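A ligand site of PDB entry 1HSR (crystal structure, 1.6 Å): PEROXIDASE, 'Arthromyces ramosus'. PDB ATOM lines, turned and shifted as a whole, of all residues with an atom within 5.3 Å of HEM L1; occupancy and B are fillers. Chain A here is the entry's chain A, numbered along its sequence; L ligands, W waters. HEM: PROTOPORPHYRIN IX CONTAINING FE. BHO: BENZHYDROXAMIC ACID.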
ATOM      1  N   SER A  45      -9.502  23.279 -25.047  1.00  0.00           N
ATOM      2  CA  SER A  45      -9.253  23.549 -23.645  1.00  0.00           C
ATOM      3  C   SER A  45     -10.420  23.280 -22.691  1.00  0.00           C
ATOM      4  O   SER A  45     -10.119  22.682 -21.637  1.00  0.00           O
ATOM      5  CB  SER A  45      -8.755  25.023 -23.502  1.00  0.00           C
ATOM      6  OG  SER A  45      -8.344  25.355 -22.191  1.00  0.00           O
ATOM      7  N   ARG A  48     -10.233  19.631 -21.587  1.00  0.00           N
ATOM      8  CA  ARG A  48      -9.032  19.342 -20.803  1.00  0.00           C
ATOM      9  C   ARG A  48      -9.157  19.917 -19.406  1.00  0.00           C
ATOM     10  O   ARG A  48      -8.822  19.257 -18.434  1.00  0.00           O
ATOM     11  CB  ARG A  48      -7.809  19.920 -21.551  1.00  0.00           C
ATOM     12  CG  ARG A  48      -7.660  19.401 -22.994  1.00  0.00           C
ATOM     13  CD  ARG A  48      -6.280  19.646 -23.550  1.00  0.00           C
ATOM     14  NE  ARG A  48      -5.925  21.068 -23.496  1.00  0.00           N
ATOM     15  CZ  ARG A  48      -6.068  21.897 -24.529  1.00  0.00           C
ATOM     16  NH1 ARG A  48      -6.580  21.497 -25.698  1.00  0.00           N
ATOM     17  NH2 ARG A  48      -5.693  23.177 -24.359  1.00  0.00           N
ATOM     18  N   LYS A  49      -9.746  21.097 -19.233  1.00  0.00           N
ATOM     19  CA  LYS A  49      -9.933  21.715 -17.923  1.00  0.00           C
ATOM     20  C   LYS A  49     -10.973  20.903 -17.146  1.00  0.00           C
ATOM     21  O   LYS A  49     -10.773  20.705 -15.935  1.00  0.00           O
ATOM     22  CB  LYS A  49     -10.426  23.154 -18.046  1.00  0.00           C
ATOM     23  CG  LYS A  49      -9.477  24.155 -18.706  1.00  0.00           C
ATOM     24  CD  LYS A  49      -8.289  24.403 -17.790  1.00  0.00           C
ATOM     25  CE  LYS A  49      -7.446  25.534 -18.316  1.00  0.00           C
ATOM     26  NZ  LYS A  49      -6.378  25.858 -17.373  1.00  0.00           N
ATOM     27  N   LEU A  51     -11.593  17.714 -17.368  1.00  0.00           N
ATOM     28  CA  LEU A  51     -10.971  16.467 -16.921  1.00  0.00           C
ATOM     29  C   LEU A  51     -10.088  16.676 -15.675  1.00  0.00           C
ATOM     30  O   LEU A  51     -10.047  15.847 -14.744  1.00  0.00           O
ATOM     31  CB  LEU A  51     -10.117  15.846 -18.032  1.00  0.00           C
ATOM     32  CG  LEU A  51     -10.829  15.049 -19.103  1.00  0.00           C
ATOM     33  CD1 LEU A  51      -9.857  14.719 -20.226  1.00  0.00           C
ATOM     34  CD2 LEU A  51     -11.417  13.779 -18.477  1.00  0.00           C
ATOM     35  N   ARG A  52      -9.376  17.815 -15.616  1.00  0.00           N
ATOM     36  CA  ARG A  52      -8.581  18.138 -14.450  1.00  0.00           C
ATOM     37  C   ARG A  52      -9.560  18.424 -13.301  1.00  0.00           C
ATOM     38  O   ARG A  52      -9.335  17.974 -12.170  1.00  0.00           O
ATOM     39  CB  ARG A  52      -7.715  19.348 -14.797  1.00  0.00           C
ATOM     40  CG  ARG A  52      -6.633  19.682 -13.791  1.00  0.00           C
ATOM     41  CD  ARG A  52      -5.640  20.645 -14.419  1.00  0.00           C
ATOM     42  NE  ARG A  52      -4.980  21.233 -13.292  1.00  0.00           N
ATOM     43  CZ  ARG A  52      -4.774  22.549 -13.213  1.00  0.00           C
ATOM     44  NH1 ARG A  52      -5.149  23.405 -14.170  1.00  0.00           N
ATOM     45  NH2 ARG A  52      -4.277  23.028 -12.063  1.00  0.00           N
ATOM     46  N   VAL A  54     -12.678  17.127 -12.715  1.00  0.00           N
ATOM     47  CA  VAL A  54     -13.358  15.957 -12.172  1.00  0.00           C
ATOM     48  C   VAL A  54     -12.419  15.200 -11.225  1.00  0.00           C
ATOM     49  O   VAL A  54     -12.862  14.729 -10.161  1.00  0.00           O
ATOM     50  CB  VAL A  54     -13.883  15.060 -13.370  1.00  0.00           C
ATOM     51  CG1 VAL A  54     -12.809  14.256 -14.108  1.00  0.00           C
ATOM     52  CG2 VAL A  54     -14.931  14.134 -12.751  1.00  0.00           C
ATOM     53  N   PHE A  55     -11.119  15.117 -11.578  1.00  0.00           N
ATOM     54  CA  PHE A  55     -10.126  14.490 -10.736  1.00  0.00           C
ATOM     55  C   PHE A  55     -10.023  15.311  -9.426  1.00  0.00           C
ATOM     56  O   PHE A  55     -10.132  14.731  -8.344  1.00  0.00           O
ATOM     57  CB  PHE A  55      -8.755  14.455 -11.466  1.00  0.00           C
ATOM     58  CG  PHE A  55      -7.601  13.879 -10.627  1.00  0.00           C
ATOM     59  CD1 PHE A  55      -7.800  12.726  -9.850  1.00  0.00           C
ATOM     60  CD2 PHE A  55      -6.349  14.493 -10.637  1.00  0.00           C
ATOM     61  CE1 PHE A  55      -6.752  12.200  -9.099  1.00  0.00           C
ATOM     62  CE2 PHE A  55      -5.301  13.959  -9.881  1.00  0.00           C
ATOM     63  CZ  PHE A  55      -5.491  12.813  -9.113  1.00  0.00           C
ATOM     64  N   PRO A 154      -2.560  15.022  -5.581  1.00  0.00           N
ATOM     65  CA  PRO A 154      -1.180  14.749  -6.006  1.00  0.00           C
ATOM     66  C   PRO A 154      -0.602  15.878  -6.866  1.00  0.00           C
ATOM     67  O   PRO A 154      -1.294  16.469  -7.719  1.00  0.00           O
ATOM     68  CB  PRO A 154      -1.253  13.455  -6.766  1.00  0.00           C
ATOM     69  CG  PRO A 154      -2.479  12.761  -6.271  1.00  0.00           C
ATOM     70  CD  PRO A 154      -3.445  13.910  -5.947  1.00  0.00           C
ATOM     71  N   GLY A 155       0.691  16.146  -6.678  1.00  0.00           N
ATOM     72  CA  GLY A 155       1.392  17.181  -7.425  1.00  0.00           C
ATOM     73  C   GLY A 155       2.503  16.594  -8.292  1.00  0.00           C
ATOM     74  O   GLY A 155       3.013  15.505  -8.011  1.00  0.00           O
ATOM     75  N   PRO A 156       2.964  17.290  -9.356  1.00  0.00           N
ATOM     76  CA  PRO A 156       3.980  16.828 -10.279  1.00  0.00           C
ATOM     77  C   PRO A 156       5.396  16.639  -9.718  1.00  0.00           C
ATOM     78  O   PRO A 156       6.241  15.983 -10.342  1.00  0.00           O
ATOM     79  CB  PRO A 156       3.945  17.831 -11.399  1.00  0.00           C
ATOM     80  CG  PRO A 156       3.601  19.121 -10.698  1.00  0.00           C
ATOM     81  CD  PRO A 156       2.552  18.636  -9.694  1.00  0.00           C
ATOM     82  N   ILE A 163       2.555   9.573  -4.370  1.00  0.00           N
ATOM     83  CA  ILE A 163       1.380   9.509  -5.234  1.00  0.00           C
ATOM     84  C   ILE A 163       0.633   8.205  -4.971  1.00  0.00           C
ATOM     85  O   ILE A 163      -0.584   8.231  -4.761  1.00  0.00           O
ATOM     86  CB  ILE A 163       1.833   9.610  -6.700  1.00  0.00           C
ATOM     87  CG1 ILE A 163       2.437  10.996  -6.963  1.00  0.00           C
ATOM     88  CG2 ILE A 163       0.647   9.344  -7.606  1.00  0.00           C
ATOM     89  CD1 ILE A 163       3.108  11.165  -8.335  1.00  0.00           C
ATOM     90  N   MET A 167      -3.275   8.065  -3.551  1.00  0.00           N
ATOM     91  CA  MET A 167      -4.250   7.422  -4.424  1.00  0.00           C
ATOM     92  C   MET A 167      -4.735   6.118  -3.809  1.00  0.00           C
ATOM     93  O   MET A 167      -5.919   5.774  -3.937  1.00  0.00           O
ATOM     94  CB  MET A 167      -3.622   7.125  -5.807  1.00  0.00           C
ATOM     95  CG  MET A 167      -3.252   8.374  -6.632  1.00  0.00           C
ATOM     96  SD  MET A 167      -4.660   9.412  -7.086  1.00  0.00           S
ATOM     97  CE  MET A 167      -5.211   8.563  -8.542  1.00  0.00           C
ATOM     98  N   VAL A 177      -3.994   3.744 -10.970  1.00  0.00           N
ATOM     99  CA  VAL A 177      -3.360   5.051 -11.081  1.00  0.00           C
ATOM    100  C   VAL A 177      -2.819   5.160 -12.516  1.00  0.00           C
ATOM    101  O   VAL A 177      -3.076   6.163 -13.171  1.00  0.00           O
ATOM    102  CB  VAL A 177      -2.179   5.228 -10.083  1.00  0.00           C
ATOM    103  CG1 VAL A 177      -1.421   6.559 -10.382  1.00  0.00           C
ATOM    104  CG2 VAL A 177      -2.720   5.183  -8.654  1.00  0.00           C
ATOM    105  N   LEU A 180      -5.882   5.684 -14.906  1.00  0.00           N
ATOM    106  CA  LEU A 180      -6.451   7.020 -14.804  1.00  0.00           C
ATOM    107  C   LEU A 180      -5.663   8.082 -15.572  1.00  0.00           C
ATOM    108  O   LEU A 180      -6.230   9.028 -16.133  1.00  0.00           O
ATOM    109  CB  LEU A 180      -6.533   7.400 -13.331  1.00  0.00           C
ATOM    110  CG  LEU A 180      -7.842   7.761 -12.581  1.00  0.00           C
ATOM    111  CD1 LEU A 180      -9.118   7.222 -13.176  1.00  0.00           C
ATOM    112  CD2 LEU A 180      -7.634   7.217 -11.190  1.00  0.00           C
ATOM    113  N   LEU A 181      -4.349   7.913 -15.652  1.00  0.00           N
ATOM    114  CA  LEU A 181      -3.458   8.838 -16.323  1.00  0.00           C
ATOM    115  C   LEU A 181      -3.576   8.799 -17.858  1.00  0.00           C
ATOM    116  O   LEU A 181      -2.924   9.591 -18.549  1.00  0.00           O
ATOM    117  CB  LEU A 181      -2.051   8.516 -15.870  1.00  0.00           C
ATOM    118  CG  LEU A 181      -1.157   9.536 -15.197  1.00  0.00           C
ATOM    119  CD1 LEU A 181      -1.847  10.850 -14.884  1.00  0.00           C
ATOM    120  CD2 LEU A 181      -0.618   8.847 -13.990  1.00  0.00           C
ATOM    121  N   ALA A 183      -5.879  10.098 -19.248  1.00  0.00           N
ATOM    122  CA  ALA A 183      -6.376  11.434 -19.485  1.00  0.00           C
ATOM    123  C   ALA A 183      -5.265  12.399 -19.877  1.00  0.00           C
ATOM    124  O   ALA A 183      -5.557  13.409 -20.513  1.00  0.00           O
ATOM    125  CB  ALA A 183      -7.052  11.979 -18.229  1.00  0.00           C
ATOM    126  N   HIS A 184      -3.969  12.098 -19.637  1.00  0.00           N
ATOM    127  CA  HIS A 184      -2.890  12.973 -20.092  1.00  0.00           C
ATOM    128  C   HIS A 184      -2.641  12.833 -21.594  1.00  0.00           C
ATOM    129  O   HIS A 184      -1.801  13.522 -22.197  1.00  0.00           O
ATOM    130  CB  HIS A 184      -1.619  12.687 -19.289  1.00  0.00           C
ATOM    131  CG  HIS A 184      -1.618  13.395 -17.928  1.00  0.00           C
ATOM    132  ND1 HIS A 184      -0.462  13.538 -17.173  1.00  0.00           N
ATOM    133  CD2 HIS A 184      -2.696  14.041 -17.301  1.00  0.00           C
ATOM    134  CE1 HIS A 184      -0.846  14.282 -16.128  1.00  0.00           C
ATOM    135  NE2 HIS A 184      -2.100  14.614 -16.176  1.00  0.00           N
ATOM    136  N   LEU A 186      -4.960  13.762 -23.540  1.00  0.00           N
ATOM    137  CA  LEU A 186      -5.763  14.915 -24.001  1.00  0.00           C
ATOM    138  C   LEU A 186      -5.317  16.055 -23.092  1.00  0.00           C
ATOM    139  O   LEU A 186      -6.137  16.601 -22.333  1.00  0.00           O
ATOM    140  CB  LEU A 186      -7.226  14.553 -23.760  1.00  0.00           C
ATOM    141  CG  LEU A 186      -8.261  14.094 -24.797  1.00  0.00           C
ATOM    142  CD1 LEU A 186      -7.643  13.583 -26.045  1.00  0.00           C
ATOM    143  CD2 LEU A 186      -9.205  13.151 -24.067  1.00  0.00           C
ATOM    144  N   ALA A 187      -4.048  16.463 -23.134  1.00  0.00           N
ATOM    145  CA  ALA A 187      -3.544  17.384 -22.133  1.00  0.00           C
ATOM    146  C   ALA A 187      -2.420  18.313 -22.528  1.00  0.00           C
ATOM    147  O   ALA A 187      -1.597  18.010 -23.406  1.00  0.00           O
ATOM    148  CB  ALA A 187      -3.060  16.586 -20.937  1.00  0.00           C
ATOM    149  N   SER A 188      -2.372  19.422 -21.823  1.00  0.00           N
ATOM    150  CA  SER A 188      -1.300  20.376 -21.986  1.00  0.00           C
ATOM    151  C   SER A 188      -1.065  20.910 -20.571  1.00  0.00           C
ATOM    152  O   SER A 188      -1.707  20.496 -19.575  1.00  0.00           O
ATOM    153  CB  SER A 188      -1.729  21.509 -22.923  1.00  0.00           C
ATOM    154  OG  SER A 188      -2.645  22.428 -22.326  1.00  0.00           O
ATOM    155  N   GLN A 189      -0.066  21.788 -20.433  1.00  0.00           N
ATOM    156  CA  GLN A 189       0.102  22.489 -19.168  1.00  0.00           C
ATOM    157  C   GLN A 189       0.028  24.004 -19.468  1.00  0.00           C
ATOM    158  O   GLN A 189       0.390  24.472 -20.554  1.00  0.00           O
ATOM    159  CB  GLN A 189       1.454  22.164 -18.517  1.00  0.00           C
ATOM    160  CG  GLN A 189       2.717  22.545 -19.279  1.00  0.00           C
ATOM    161  CD  GLN A 189       3.164  24.004 -19.161  1.00  0.00           C
ATOM    162  OE1 GLN A 189       2.958  24.658 -18.133  1.00  0.00           O
ATOM    163  NE2 GLN A 189       3.775  24.549 -20.205  1.00  0.00           N
ATOM    164  N   GLU A 190      -0.387  24.799 -18.521  1.00  0.00           N
ATOM    165  CA  GLU A 190      -0.452  26.244 -18.671  1.00  0.00           C
ATOM    166  C   GLU A 190       0.315  26.967 -17.596  1.00  0.00           C
ATOM    167  O   GLU A 190       0.833  28.061 -17.831  1.00  0.00           O
ATOM    168  CB  GLU A 190      -1.852  26.773 -18.582  1.00  0.00           C
ATOM    169  CG  GLU A 190      -2.674  26.429 -19.810  1.00  0.00           C
ATOM    170  CD  GLU A 190      -4.132  26.892 -19.778  1.00  0.00           C
ATOM    171  OE1 GLU A 190      -4.582  27.538 -18.832  1.00  0.00           O
ATOM    172  OE2 GLU A 190      -4.829  26.610 -20.740  1.00  0.00           O
ATOM    173  N   GLY A 191       0.377  26.361 -16.404  1.00  0.00           N
ATOM    174  CA  GLY A 191       0.954  26.999 -15.235  1.00  0.00           C
ATOM    175  C   GLY A 191       2.298  26.495 -14.760  1.00  0.00           C
ATOM    176  O   GLY A 191       2.853  27.064 -13.816  1.00  0.00           O
ATOM    177  N   LEU A 192       2.835  25.436 -15.331  1.00  0.00           N
ATOM    178  CA  LEU A 192       4.130  24.921 -14.896  1.00  0.00           C
ATOM    179  C   LEU A 192       5.254  25.672 -15.579  1.00  0.00           C
ATOM    180  O   LEU A 192       6.308  25.889 -14.979  1.00  0.00           O
ATOM    181  CB  LEU A 192       4.192  23.436 -15.224  1.00  0.00           C
ATOM    182  CG  LEU A 192       3.820  22.364 -14.202  1.00  0.00           C
ATOM    183  CD1 LEU A 192       2.784  22.800 -13.240  1.00  0.00           C
ATOM    184  CD2 LEU A 192       3.411  21.160 -14.996  1.00  0.00           C
ATOM    185  N   LEU A 201       1.238  17.324 -23.676  1.00  0.00           N
ATOM    186  CA  LEU A 201       1.897  16.231 -22.993  1.00  0.00           C
ATOM    187  C   LEU A 201       2.077  15.069 -23.981  1.00  0.00           C
ATOM    188  O   LEU A 201       2.816  14.132 -23.685  1.00  0.00           O
ATOM    189  CB  LEU A 201       1.030  15.838 -21.779  1.00  0.00           C
ATOM    190  CG  LEU A 201       1.376  16.436 -20.380  1.00  0.00           C
ATOM    191  CD1 LEU A 201       1.755  17.899 -20.469  1.00  0.00           C
ATOM    192  CD2 LEU A 201       0.230  16.148 -19.443  1.00  0.00           C
ATOM    193  N   MET A 243       6.268  16.242 -17.550  1.00  0.00           N
ATOM    194  CA  MET A 243       6.344  16.561 -16.124  1.00  0.00           C
ATOM    195  C   MET A 243       6.982  15.375 -15.377  1.00  0.00           C
ATOM    196  O   MET A 243       6.908  14.212 -15.811  1.00  0.00           O
ATOM    197  CB  MET A 243       4.939  16.882 -15.511  1.00  0.00           C
ATOM    198  CG  MET A 243       3.881  15.823 -15.513  1.00  0.00           C
ATOM    199  SD  MET A 243       2.359  16.355 -14.671  1.00  0.00           S
ATOM    200  CE  MET A 243       1.701  14.795 -14.369  1.00  0.00           C
ATOM    201  N   SER A 245       6.399  13.677 -12.442  1.00  0.00           N
ATOM    202  CA  SER A 245       5.619  12.546 -12.012  1.00  0.00           C
ATOM    203  C   SER A 245       5.315  11.565 -13.154  1.00  0.00           C
ATOM    204  O   SER A 245       5.450  10.351 -12.951  1.00  0.00           O
ATOM    205  CB  SER A 245       4.359  13.088 -11.377  1.00  0.00           C
ATOM    206  OG  SER A 245       3.657  13.992 -12.207  1.00  0.00           O
ATOM    207  N   LEU A 249       6.618   7.776 -13.054  1.00  0.00           N
ATOM    208  CA  LEU A 249       5.660   6.671 -13.045  1.00  0.00           C
ATOM    209  C   LEU A 249       5.928   5.750 -14.208  1.00  0.00           C
ATOM    210  O   LEU A 249       5.779   4.532 -14.076  1.00  0.00           O
ATOM    211  CB  LEU A 249       4.210   7.217 -13.116  1.00  0.00           C
ATOM    212  CG  LEU A 249       3.734   7.889 -11.826  1.00  0.00           C
ATOM    213  CD1 LEU A 249       2.476   8.670 -12.071  1.00  0.00           C
ATOM    214  CD2 LEU A 249       3.473   6.844 -10.762  1.00  0.00           C
ATOM    215  N   TYR A 273      -9.419   2.670 -18.800  1.00  0.00           N
ATOM    216  CA  TYR A 273      -9.718   4.030 -18.366  1.00  0.00           C
ATOM    217  C   TYR A 273     -11.201   4.163 -18.008  1.00  0.00           C
ATOM    218  O   TYR A 273     -11.545   4.757 -16.975  1.00  0.00           O
ATOM    219  CB  TYR A 273      -9.344   5.023 -19.478  1.00  0.00           C
ATOM    220  CG  TYR A 273      -9.719   6.469 -19.196  1.00  0.00           C
ATOM    221  CD1 TYR A 273      -8.961   7.252 -18.292  1.00  0.00           C
ATOM    222  CD2 TYR A 273     -10.801   7.037 -19.881  1.00  0.00           C
ATOM    223  CE1 TYR A 273      -9.300   8.592 -18.070  1.00  0.00           C
ATOM    224  CE2 TYR A 273     -11.137   8.371 -19.671  1.00  0.00           C
ATOM    225  CZ  TYR A 273     -10.384   9.141 -18.770  1.00  0.00           C
ATOM    226  OH  TYR A 273     -10.701  10.464 -18.606  1.00  0.00           O
ATOM    227  N   MET A 277     -12.507   5.384 -14.239  1.00  0.00           N
ATOM    228  CA  MET A 277     -13.322   6.599 -14.132  1.00  0.00           C
ATOM    229  C   MET A 277     -14.672   6.331 -13.492  1.00  0.00           C
ATOM    230  O   MET A 277     -15.193   7.170 -12.735  1.00  0.00           O
ATOM    231  CB  MET A 277     -13.573   7.217 -15.507  1.00  0.00           C
ATOM    232  CG  MET A 277     -12.329   7.910 -16.094  1.00  0.00           C
ATOM    233  SD  MET A 277     -11.721   9.329 -15.113  1.00  0.00           S
ATOM    234  CE  MET A 277     -12.938  10.517 -15.644  1.00  0.00           C
ATOM    235  N   MET A 280     -13.952   6.257  -9.836  1.00  0.00           N
ATOM    236  CA  MET A 280     -13.710   7.594  -9.317  1.00  0.00           C
ATOM    237  C   MET A 280     -14.982   8.431  -9.228  1.00  0.00           C
ATOM    238  O   MET A 280     -15.110   9.224  -8.288  1.00  0.00           O
ATOM    239  CB  MET A 280     -12.682   8.325 -10.188  1.00  0.00           C
ATOM    240  CG  MET A 280     -12.294   9.709  -9.634  1.00  0.00           C
ATOM    241  SD  MET A 280     -10.762  10.357 -10.337  1.00  0.00           S
ATOM    242  CE  MET A 280     -11.573  11.037 -11.738  1.00  0.00           C
HETATM  243  CHA HEM L   1      -2.776  18.523 -16.563  1.00  0.00           C
HETATM  244  CHB HEM L   1      -0.643  16.721 -12.641  1.00  0.00           C
HETATM  245  CHC HEM L   1      -3.626  12.953 -12.813  1.00  0.00           C
HETATM  246  CHD HEM L   1      -6.215  15.173 -16.151  1.00  0.00           C
HETATM  247  C1A HEM L   1      -1.932  18.355 -15.484  1.00  0.00           C
HETATM  248  C2A HEM L   1      -0.977  19.348 -15.048  1.00  0.00           C
HETATM  249  C3A HEM L   1      -0.387  18.849 -13.912  1.00  0.00           C
HETATM  250  C4A HEM L   1      -1.006  17.580 -13.661  1.00  0.00           C
HETATM  251  CMA HEM L   1       0.724  19.468 -13.078  1.00  0.00           C
HETATM  252  CAA HEM L   1      -0.784  20.687 -15.723  1.00  0.00           C
HETATM  253  CBA HEM L   1      -1.685  21.766 -15.143  1.00  0.00           C
HETATM  254  CGA HEM L   1      -1.335  23.122 -15.709  1.00  0.00           C
HETATM  255  O1A HEM L   1      -2.070  23.623 -16.538  1.00  0.00           O
HETATM  256  O2A HEM L   1      -0.289  23.677 -15.350  1.00  0.00           O
HETATM  257  C1B HEM L   1      -1.192  15.464 -12.416  1.00  0.00           C
HETATM  258  C2B HEM L   1      -0.726  14.535 -11.389  1.00  0.00           C
HETATM  259  C3B HEM L   1      -1.581  13.461 -11.439  1.00  0.00           C
HETATM  260  C4B HEM L   1      -2.512  13.732 -12.528  1.00  0.00           C
HETATM  261  CMB HEM L   1       0.500  14.723 -10.506  1.00  0.00           C
HETATM  262  CAB HEM L   1      -1.686  12.393 -10.546  1.00  0.00           C
HETATM  263  CBB HEM L   1      -0.730  11.327 -10.459  1.00  0.00           C
HETATM  264  C1C HEM L   1      -4.637  13.262 -13.683  1.00  0.00           C
HETATM  265  C2C HEM L   1      -5.888  12.532 -13.771  1.00  0.00           C
HETATM  266  C3C HEM L   1      -6.674  13.203 -14.657  1.00  0.00           C
HETATM  267  C4C HEM L   1      -5.861  14.316 -15.126  1.00  0.00           C
HETATM  268  CMC HEM L   1      -6.204  11.281 -12.955  1.00  0.00           C
HETATM  269  CAC HEM L   1      -8.020  13.005 -14.992  1.00  0.00           C
HETATM  270  CBC HEM L   1      -8.701  11.718 -15.124  1.00  0.00           C
HETATM  271  C1D HEM L   1      -5.423  16.215 -16.648  1.00  0.00           C
HETATM  272  C2D HEM L   1      -5.722  16.947 -17.881  1.00  0.00           C
HETATM  273  C3D HEM L   1      -4.763  17.898 -17.952  1.00  0.00           C
HETATM  274  C4D HEM L   1      -3.863  17.702 -16.844  1.00  0.00           C
HETATM  275  CMD HEM L   1      -6.766  16.571 -18.929  1.00  0.00           C
HETATM  276  CAD HEM L   1      -4.632  18.964 -19.006  1.00  0.00           C
HETATM  277  CBD HEM L   1      -5.272  20.308 -18.637  1.00  0.00           C
HETATM  278  CGD HEM L   1      -5.105  21.350 -19.743  1.00  0.00           C
HETATM  279  O1D HEM L   1      -5.482  22.493 -19.508  1.00  0.00           O
HETATM  280  O2D HEM L   1      -4.642  21.030 -20.844  1.00  0.00           O
HETATM  281  NA  HEM L   1      -1.967  17.290 -14.614  1.00  0.00           N
HETATM  282  NB  HEM L   1      -2.249  14.943 -13.128  1.00  0.00           N
HETATM  283  NC  HEM L   1      -4.643  14.366 -14.495  1.00  0.00           N
HETATM  284  ND  HEM L   1      -4.239  16.633 -16.085  1.00  0.00           N
HETATM  285 FE   HEM L   1      -3.205  15.743 -14.655  1.00  0.00          FE
HETATM  286  C1  BHO L   2      -1.428  19.927  -9.876  1.00  0.00           C
HETATM  287  C2  BHO L   2      -1.031  21.051 -10.639  1.00  0.00           C
HETATM  288  C3  BHO L   2      -0.074  21.952 -10.142  1.00  0.00           C
HETATM  289  C4  BHO L   2       0.497  21.739  -8.883  1.00  0.00           C
HETATM  290  C5  BHO L   2       0.096  20.629  -8.112  1.00  0.00           C
HETATM  291  C6  BHO L   2      -0.855  19.733  -8.601  1.00  0.00           C
HETATM  292  C   BHO L   2      -2.384  19.046 -10.423  1.00  0.00           C
HETATM  293  O1  BHO L   2      -3.082  19.378 -11.411  1.00  0.00           O
HETATM  294  N   BHO L   2      -2.529  17.832  -9.861  1.00  0.00           N
HETATM  295  O2  BHO L   2      -3.488  17.050 -10.499  1.00  0.00           O
HETATM  296  O   HOH W   1      -3.474  25.886 -15.186  1.00  0.00           O
HETATM  297  O   HOH W   2      -5.904  24.094 -21.584  1.00  0.00           O
HETATM  298  O   HOH W   3      -4.619  17.189 -12.832  1.00  0.00           O
HETATM  299  O   HOH W   4      -1.300  25.184 -12.711  1.00  0.00           O
HETATM  300  O   HOH W   5      -4.814  23.445 -17.013  1.00  0.00           O
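The side-chain hydroxyl of Ser 188 lies within hydrogen-bond range of an oxygen (O2D) of HEM L1 (2.9 Å).
An oxygen (O2A) of HEM L1 sits at hydrogen-bond distance from the backbone NH of Gly 191.
An oxygen (O1) of BHO L2 is in hydrogen-bond range of the guanidinium group (NE) of Arg 52, 3.3 Å away.
An oxygen (O1A) of HEM L1 lies within hydrogen-bond range of the backbone NH of Glu 190, at 2.9 Å.
O2D of HEM L1 lies within hydrogen-bond range of N of Ser 188 (2.9 Å).
The guanidinium group (NE) of Arg 48 lies within salt-bridge range of an oxygen (O2D) of HEM L1 (2.9 Å).
An oxygen (O1A) of HEM L1 is in salt-bridge range of the guanidinium group (NH1) of Arg 52 (3.9 Å).
A ring nitrogen (NE2) of His 184 is bound to an iron atom (FE) of HEM L1 (2.2 Å).
O of Pro 154 sits at hydrogen-bond distance from N of BHO L2 (2.8 Å).
The side-chain carboxylate of Glu 190 is in salt-bridge range of the side-chain amino group of Lys 49, at 2.9 Å.
The backbone NH (N) of Leu 192 sits at hydrogen-bond distance from the side-chain amide oxygen (OE1) of Gln 189 (2.9 Å).
O of Ala 187 is in hydrogen-bond range of N of Leu 201, 2.9 Å away.
N of Ser 245 is in hydrogen-bond range of O of Pro 156 (3.1 Å).
SD of Met 243 sits close to OG of Ser 245 (3.7 Å).
Merely in contact with HEM L1: Lys 49, Leu 51, Phe 55, Pro 154, Gly 155, Pro 156, Ile 163, Leu 180, Leu 181, Ala 183, Leu 186, Ala 187, Gln 189, Leu 192, Met 243, Ser 245 and Met 277.
Hydrophobic or aromatic side chains within 4 Å of HEM L1: Leu 51, Phe 55, Pro 154, Pro 156, Ile 163, Leu 180, Leu 181, Ala 183, His 184, Ala 187, Leu 192, Met 243 and Met 277.
Of the 31 residues printed, 23 come within 4 Å of HEM L1.
Along chain A the residues within 4 Å of HEM L1 span positions 48 to 277.
Water W2 lies within hydrogen-bond range of O1D of HEM L1 (2.7 Å), OG of Ser 45 (2.8 Å), OE2 of Glu 190 (2.9 Å) and NH2 of Arg 48 (2.9 Å).
Water W5 lies within hydrogen-bond range of an oxygen (O1D) of HEM L1 (2.8 Å), the guanidinium group of Arg 52 (2.9 Å) and the side-chain amino group of Lys 49 (2.9 Å).
Water W1 lies within hydrogen-bond range of an oxygen (O1A) of HEM L1 (3.0 Å) and the guanidinium group of Arg 52 (3.2 Å).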
